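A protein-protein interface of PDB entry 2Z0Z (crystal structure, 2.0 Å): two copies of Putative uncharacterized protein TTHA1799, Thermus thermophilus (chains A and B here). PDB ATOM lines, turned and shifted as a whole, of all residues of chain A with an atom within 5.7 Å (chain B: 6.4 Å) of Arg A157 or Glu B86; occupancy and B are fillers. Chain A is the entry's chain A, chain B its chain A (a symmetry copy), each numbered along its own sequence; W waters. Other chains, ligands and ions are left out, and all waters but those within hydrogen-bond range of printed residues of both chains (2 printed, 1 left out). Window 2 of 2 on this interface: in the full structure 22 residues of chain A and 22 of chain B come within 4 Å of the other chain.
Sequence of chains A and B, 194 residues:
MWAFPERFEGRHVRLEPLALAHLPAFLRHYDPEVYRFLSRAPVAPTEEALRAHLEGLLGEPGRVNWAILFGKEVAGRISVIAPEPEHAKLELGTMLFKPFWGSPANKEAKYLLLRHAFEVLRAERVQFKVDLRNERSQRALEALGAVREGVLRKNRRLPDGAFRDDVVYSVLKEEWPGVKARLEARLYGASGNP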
ATOM      1  N   ASN A 155      -4.945   1.319 -15.902  1.00  0.00           N
ATOM      2  CA  ASN A 155      -5.149   0.234 -16.844  1.00  0.00           C
ATOM      3  C   ASN A 155      -4.271  -0.990 -16.644  1.00  0.00           C
ATOM      4  O   ASN A 155      -4.535  -2.035 -17.231  1.00  0.00           O
ATOM      5  CB  ASN A 155      -5.013   0.763 -18.267  1.00  0.00           C
ATOM      6  CG  ASN A 155      -5.631  -0.172 -19.277  1.00  0.00           C
ATOM      7  OD1 ASN A 155      -6.784  -0.584 -19.124  1.00  0.00           O
ATOM      8  ND2 ASN A 155      -4.875  -0.517 -20.308  1.00  0.00           N
ATOM      9  N   ARG A 156      -3.225  -0.879 -15.826  1.00  0.00           N
ATOM     10  CA  ARG A 156      -2.381  -2.033 -15.561  1.00  0.00           C
ATOM     11  C   ARG A 156      -1.853  -1.935 -14.154  1.00  0.00           C
ATOM     12  O   ARG A 156      -1.771  -0.843 -13.592  1.00  0.00           O
ATOM     13  CB  ARG A 156      -1.200  -2.123 -16.546  1.00  0.00           C
ATOM     14  CG  ARG A 156      -0.101  -1.074 -16.361  1.00  0.00           C
ATOM     15  CD  ARG A 156       0.983  -1.207 -17.459  1.00  0.00           C
ATOM     16  NE  ARG A 156       2.070  -0.233 -17.336  1.00  0.00           N
ATOM     17  CZ  ARG A 156       3.316  -0.540 -16.969  1.00  0.00           C
ATOM     18  NH1 ARG A 156       3.632  -1.800 -16.679  1.00  0.00           N
ATOM     19  NH2 ARG A 156       4.260   0.403 -16.923  1.00  0.00           N
ATOM     20  N   ARG A 157      -1.511  -3.082 -13.581  1.00  0.00           N
ATOM     21  CA  ARG A 157      -0.985  -3.123 -12.224  1.00  0.00           C
ATOM     22  C   ARG A 157       0.414  -3.699 -12.272  1.00  0.00           C
ATOM     23  O   ARG A 157       0.683  -4.603 -13.063  1.00  0.00           O
ATOM     24  CB  ARG A 157      -1.864  -4.002 -11.330  1.00  0.00           C
ATOM     25  CG  ARG A 157      -1.529  -3.864  -9.864  1.00  0.00           C
ATOM     26  CD  ARG A 157      -2.503  -4.605  -8.967  1.00  0.00           C
ATOM     27  NE  ARG A 157      -2.542  -3.949  -7.666  1.00  0.00           N
ATOM     28  CZ  ARG A 157      -3.313  -4.312  -6.644  1.00  0.00           C
ATOM     29  NH1 ARG A 157      -4.136  -5.357  -6.753  1.00  0.00           N
ATOM     30  NH2 ARG A 157      -3.270  -3.608  -5.516  1.00  0.00           N
ATOM     31  N   LEU A 158       1.302  -3.161 -11.440  1.00  0.00           N
ATOM     32  CA  LEU A 158       2.697  -3.625 -11.371  1.00  0.00           C
ATOM     33  C   LEU A 158       2.859  -4.720 -10.313  1.00  0.00           C
ATOM     34  O   LEU A 158       2.006  -4.880  -9.442  1.00  0.00           O
ATOM     35  CB  LEU A 158       3.617  -2.457 -11.005  1.00  0.00           C
ATOM     36  CG  LEU A 158       3.510  -1.206 -11.876  1.00  0.00           C
ATOM     37  CD1 LEU A 158       4.545  -0.184 -11.423  1.00  0.00           C
ATOM     38  CD2 LEU A 158       3.733  -1.579 -13.329  1.00  0.00           C
ATOM     39  N   PRO A 159       3.971  -5.479 -10.364  1.00  0.00           N
ATOM     40  CA  PRO A 159       4.152  -6.532  -9.363  1.00  0.00           C
ATOM     41  C   PRO A 159       4.067  -6.032  -7.915  1.00  0.00           C
ATOM     42  O   PRO A 159       3.583  -6.754  -7.057  1.00  0.00           O
ATOM     43  CB  PRO A 159       5.532  -7.111  -9.709  1.00  0.00           C
ATOM     44  CG  PRO A 159       5.587  -6.942 -11.205  1.00  0.00           C
ATOM     45  CD  PRO A 159       5.044  -5.528 -11.381  1.00  0.00           C
ATOM     46  N   GLY A 161       2.088  -3.995  -6.783  1.00  0.00           N
ATOM     47  CA  GLY A 161       0.732  -3.575  -6.472  1.00  0.00           C
ATOM     48  C   GLY A 161       0.328  -2.182  -6.904  1.00  0.00           C
ATOM     49  O   GLY A 161      -0.844  -1.822  -6.797  1.00  0.00           O
ATOM     50  N   ALA A 162       1.271  -1.386  -7.389  1.00  0.00           N
ATOM     51  CA  ALA A 162       0.934  -0.036  -7.820  1.00  0.00           C
ATOM     52  C   ALA A 162       0.273  -0.085  -9.199  1.00  0.00           C
ATOM     53  O   ALA A 162       0.475  -1.036  -9.948  1.00  0.00           O
ATOM     54  CB  ALA A 162       2.180   0.836  -7.876  1.00  0.00           C
ATOM     55  N   PHE A 163      -0.504   0.949  -9.513  1.00  0.00           N
ATOM     56  CA  PHE A 163      -1.199   1.065 -10.798  1.00  0.00           C
ATOM     57  C   PHE A 163      -0.579   2.127 -11.711  1.00  0.00           C
ATOM     58  O   PHE A 163       0.034   3.077 -11.242  1.00  0.00           O
ATOM     59  CB  PHE A 163      -2.670   1.413 -10.558  1.00  0.00           C
ATOM     60  CG  PHE A 163      -3.456   0.307  -9.939  1.00  0.00           C
ATOM     61  CD1 PHE A 163      -4.025  -0.693 -10.735  1.00  0.00           C
ATOM     62  CD2 PHE A 163      -3.618   0.244  -8.554  1.00  0.00           C
ATOM     63  CE1 PHE A 163      -4.744  -1.738 -10.166  1.00  0.00           C
ATOM     64  CE2 PHE A 163      -4.336  -0.800  -7.963  1.00  0.00           C
ATOM     65  CZ  PHE A 163      -4.905  -1.801  -8.779  1.00  0.00           C
ATOM     66  N   ARG A 164      -0.721   1.943 -13.016  1.00  0.00           N
ATOM     67  CA  ARG A 164      -0.218   2.907 -13.984  1.00  0.00           C
ATOM     68  C   ARG A 164      -1.300   3.184 -15.032  1.00  0.00           C
ATOM     69  O   ARG A 164      -2.173   2.345 -15.260  1.00  0.00           O
ATOM     70  CB  ARG A 164       1.054   2.389 -14.651  1.00  0.00           C
ATOM     71  CG  ARG A 164       2.268   2.303 -13.687  1.00  0.00           C
ATOM     72  CD  ARG A 164       2.671   3.668 -13.108  1.00  0.00           C
ATOM     73  NE  ARG A 164       3.823   3.555 -12.203  1.00  0.00           N
ATOM     74  CZ  ARG A 164       3.752   3.546 -10.866  1.00  0.00           C
ATOM     75  NH1 ARG A 164       2.577   3.663 -10.244  1.00  0.00           N
ATOM     76  NH2 ARG A 164       4.864   3.379 -10.143  1.00  0.00           N
ATOM     77  N   MET B   1      -8.417 -16.771  -9.955  1.00  0.00           N
ATOM     78  CA  MET B   1      -9.498 -16.048 -10.684  1.00  0.00           C
ATOM     79  C   MET B   1     -10.517 -15.532  -9.668  1.00  0.00           C
ATOM     80  O   MET B   1     -10.510 -15.960  -8.507  1.00  0.00           O
ATOM     81  CB  MET B   1     -10.196 -16.994 -11.674  1.00  0.00           C
ATOM     82  CG  MET B   1     -11.199 -17.953 -11.054  1.00  0.00           C
ATOM     83  SD  MET B   1     -12.054 -19.010 -12.298  1.00  0.00           S
ATOM     84  CE  MET B   1     -12.944 -17.816 -13.253  1.00  0.00           C
ATOM     85  N   TRP B   2     -11.372 -14.608 -10.087  1.00  0.00           N
ATOM     86  CA  TRP B   2     -12.397 -14.111  -9.177  1.00  0.00           C
ATOM     87  C   TRP B   2     -13.564 -15.063  -9.225  1.00  0.00           C
ATOM     88  O   TRP B   2     -13.967 -15.502 -10.307  1.00  0.00           O
ATOM     89  CB  TRP B   2     -12.912 -12.745  -9.587  1.00  0.00           C
ATOM     90  CG  TRP B   2     -11.974 -11.614  -9.342  1.00  0.00           C
ATOM     91  CD1 TRP B   2     -11.059 -11.497  -8.336  1.00  0.00           C
ATOM     92  CD2 TRP B   2     -11.902 -10.400 -10.094  1.00  0.00           C
ATOM     93  NE1 TRP B   2     -10.420 -10.278  -8.416  1.00  0.00           N
ATOM     94  CE2 TRP B   2     -10.921  -9.586  -9.487  1.00  0.00           C
ATOM     95  CE3 TRP B   2     -12.572  -9.921 -11.228  1.00  0.00           C
ATOM     96  CZ2 TRP B   2     -10.594  -8.316  -9.975  1.00  0.00           C
ATOM     97  CZ3 TRP B   2     -12.241  -8.655 -11.711  1.00  0.00           C
ATOM     98  CH2 TRP B   2     -11.267  -7.872 -11.086  1.00  0.00           C
ATOM     99  N   PRO B  83     -12.527 -10.134 -17.286  1.00  0.00           N
ATOM    100  CA  PRO B  83     -12.085  -9.827 -15.928  1.00  0.00           C
ATOM    101  C   PRO B  83     -10.610 -10.212 -15.827  1.00  0.00           C
ATOM    102  O   PRO B  83     -10.201 -11.249 -16.347  1.00  0.00           O
ATOM    103  CB  PRO B  83     -12.987 -10.703 -15.055  1.00  0.00           C
ATOM    104  CG  PRO B  83     -13.237 -11.912 -15.935  1.00  0.00           C
ATOM    105  CD  PRO B  83     -13.439 -11.300 -17.318  1.00  0.00           C
ATOM    106  N   GLU B  84      -9.811  -9.348 -15.207  1.00  0.00           N
ATOM    107  CA  GLU B  84      -8.389  -9.594 -15.059  1.00  0.00           C
ATOM    108  C   GLU B  84      -7.975  -9.285 -13.638  1.00  0.00           C
ATOM    109  O   GLU B  84      -7.539  -8.164 -13.318  1.00  0.00           O
ATOM    110  CB  GLU B  84      -7.586  -8.727 -16.024  1.00  0.00           C
ATOM    111  CG  GLU B  84      -7.729  -9.139 -17.473  1.00  0.00           C
ATOM    112  CD  GLU B  84      -6.744  -8.413 -18.358  1.00  0.00           C
ATOM    113  OE1 GLU B  84      -5.520  -8.535 -18.138  1.00  0.00           O
ATOM    114  OE2 GLU B  84      -7.188  -7.716 -19.263  1.00  0.00           O
ATOM    115  N   PRO B  85      -8.117 -10.276 -12.759  1.00  0.00           N
ATOM    116  CA  PRO B  85      -7.737 -10.051 -11.370  1.00  0.00           C
ATOM    117  C   PRO B  85      -6.300  -9.584 -11.215  1.00  0.00           C
ATOM    118  O   PRO B  85      -5.999  -8.838 -10.287  1.00  0.00           O
ATOM    119  CB  PRO B  85      -8.028 -11.396 -10.683  1.00  0.00           C
ATOM    120  CG  PRO B  85      -8.185 -12.388 -11.802  1.00  0.00           C
ATOM    121  CD  PRO B  85      -8.706 -11.610 -12.970  1.00  0.00           C
ATOM    122  N   GLU B  86      -5.418  -9.977 -12.134  1.00  0.00           N
ATOM    123  CA  GLU B  86      -4.011  -9.569 -12.052  1.00  0.00           C
ATOM    124  C   GLU B  86      -3.880  -8.049 -12.118  1.00  0.00           C
ATOM    125  O   GLU B  86      -2.964  -7.465 -11.522  1.00  0.00           O
ATOM    126  CB  GLU B  86      -3.175 -10.166 -13.197  1.00  0.00           C
ATOM    127  CG  GLU B  86      -3.303 -11.677 -13.393  1.00  0.00           C
ATOM    128  CD  GLU B  86      -2.753 -12.496 -12.236  1.00  0.00           C
ATOM    129  OE1 GLU B  86      -1.515 -12.484 -12.026  1.00  0.00           O
ATOM    130  OE2 GLU B  86      -3.568 -13.158 -11.542  1.00  0.00           O
ATOM    131  N   HIS B  87      -4.781  -7.409 -12.855  1.00  0.00           N
ATOM    132  CA  HIS B  87      -4.743  -5.953 -12.976  1.00  0.00           C
ATOM    133  C   HIS B  87      -5.916  -5.292 -12.245  1.00  0.00           C
ATOM    134  O   HIS B  87      -6.192  -4.098 -12.441  1.00  0.00           O
ATOM    135  CB  HIS B  87      -4.753  -5.572 -14.462  1.00  0.00           C
ATOM    136  CG  HIS B  87      -3.540  -6.053 -15.199  1.00  0.00           C
ATOM    137  ND1 HIS B  87      -2.286  -5.524 -14.979  1.00  0.00           N
ATOM    138  CD2 HIS B  87      -3.380  -7.031 -16.124  1.00  0.00           C
ATOM    139  CE1 HIS B  87      -1.405  -6.152 -15.740  1.00  0.00           C
ATOM    140  NE2 HIS B  87      -2.043  -7.070 -16.444  1.00  0.00           N
ATOM    141  N   ALA B  88      -6.608  -6.078 -11.422  1.00  0.00           N
ATOM    142  CA  ALA B  88      -7.765  -5.586 -10.664  1.00  0.00           C
ATOM    143  C   ALA B  88      -8.739  -4.794 -11.543  1.00  0.00           C
ATOM    144  O   ALA B  88      -9.176  -3.694 -11.177  1.00  0.00           O
ATOM    145  CB  ALA B  88      -7.291  -4.710  -9.484  1.00  0.00           C
ATOM    146  N   LYS B  89      -9.082  -5.339 -12.708  1.00  0.00           N
ATOM    147  CA  LYS B  89     -10.003  -4.629 -13.590  1.00  0.00           C
ATOM    148  C   LYS B  89     -10.922  -5.564 -14.376  1.00  0.00           C
ATOM    149  O   LYS B  89     -10.650  -6.766 -14.486  1.00  0.00           O
ATOM    150  CB  LYS B  89      -9.212  -3.767 -14.584  1.00  0.00           C
ATOM    151  CG  LYS B  89      -8.387  -4.591 -15.587  1.00  0.00           C
ATOM    152  CD  LYS B  89      -7.657  -3.668 -16.565  1.00  0.00           C
ATOM    153  CE  LYS B  89      -6.901  -4.453 -17.629  1.00  0.00           C
ATOM    154  NZ  LYS B  89      -6.391  -3.523 -18.658  1.00  0.00           N
ATOM    155  N   ARG B 122     -12.403  -6.073  -4.738  1.00  0.00           N
ATOM    156  CA  ARG B 122     -11.411  -5.006  -4.730  1.00  0.00           C
ATOM    157  C   ARG B 122     -10.863  -4.611  -6.116  1.00  0.00           C
ATOM    158  O   ARG B 122      -9.676  -4.345  -6.286  1.00  0.00           O
ATOM    159  CB  ARG B 122     -10.276  -5.367  -3.760  1.00  0.00           C
ATOM    160  CG  ARG B 122     -10.781  -5.428  -2.300  1.00  0.00           C
ATOM    161  CD  ARG B 122      -9.724  -5.921  -1.302  1.00  0.00           C
ATOM    162  NE  ARG B 122      -8.674  -4.938  -1.031  1.00  0.00           N
ATOM    163  CZ  ARG B 122      -7.684  -5.113  -0.147  1.00  0.00           C
ATOM    164  NH1 ARG B 122      -7.596  -6.239   0.559  1.00  0.00           N
ATOM    165  NH2 ARG B 122      -6.781  -4.152   0.042  1.00  0.00           N
HETATM  166  O   HOH W   1      -5.123  -2.271 -13.932  1.00  0.00           O
HETATM  167  O   HOH W   2      -4.022  -7.511  -8.385  1.00  0.00           O
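ND1 of His B87 is in hydrogen-bond range of N of Arg A157 (2.9 Å). O of Asn A155 lies within hydrogen-bond range of NZ of Lys B89 (2.8 Å).
N of Glu B84 is in hydrogen-bond range of O of Lys B89 (2.8 Å). The backbone NH (N) of Arg A164 is in hydrogen-bond range of the backbone carbonyl oxygen (O) of Arg A156 (3.0 Å). The guanidinium group (NE) of Arg A157 is in hydrogen-bond range of the backbone carbonyl oxygen (O) of Gly A161, 2.9 Å away. N of Asn A155 sits at hydrogen-bond distance from O of Arg A164 (3.0 Å).
Among the printed residues, merely in contact across the chains: Arg A156 with His B87 (3.5 Å), Phe A163 with His B87 (3.6 Å), Arg A157 with Glu B86 (3.6 Å) and Phe A163 with Ala B88 (3.8 Å).
Arg A157 touches just these residues of chain B: Glu B86 and His B87. Printed residues of chain A within 4 Å of Glu B86: Arg A157. Of the printed residues of chain A, His B87 touches Arg A156 (3.5 Å), Arg A157 (2.9 Å) and Phe A163 (3.6 Å). Of the printed residues of chain A, Ala B88 touches Phe A163. Of the printed residues of chain B, Phe A163 touches His B87 and Ala B88. Printed residues of chain B within 4 Å of Arg A156: His B87 (3.5 Å). The nearest residue of chain B that does not touch Arg A157 is Ala B88 (4.2 Å).
Of the 10 printed residues of chain B, 4 touch a printed residue of chain A. Hydrophobic or aromatic side chains of chain B within 4 Å of the printed part of chain A: His B87 and Ala B88. Among the printed residues, no Asp or Glu carboxylate lies within 4 Å of a Lys or Arg side-chain nitrogen of the other chain.
No position is printed for both chains. Of the 6 pairs that touch across the chains among the printed residues, none has its exchanged pair printed and touching as well.
Water W1 lies within hydrogen-bond range of O of His B87 (2.6 Å), N of Arg A156 (3.0 Å) and O of Asn A155 (3.4 Å). Water W2 lies within hydrogen-bond range of NH1 of Arg A157, O of Pro B85 and O of Glu B86.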
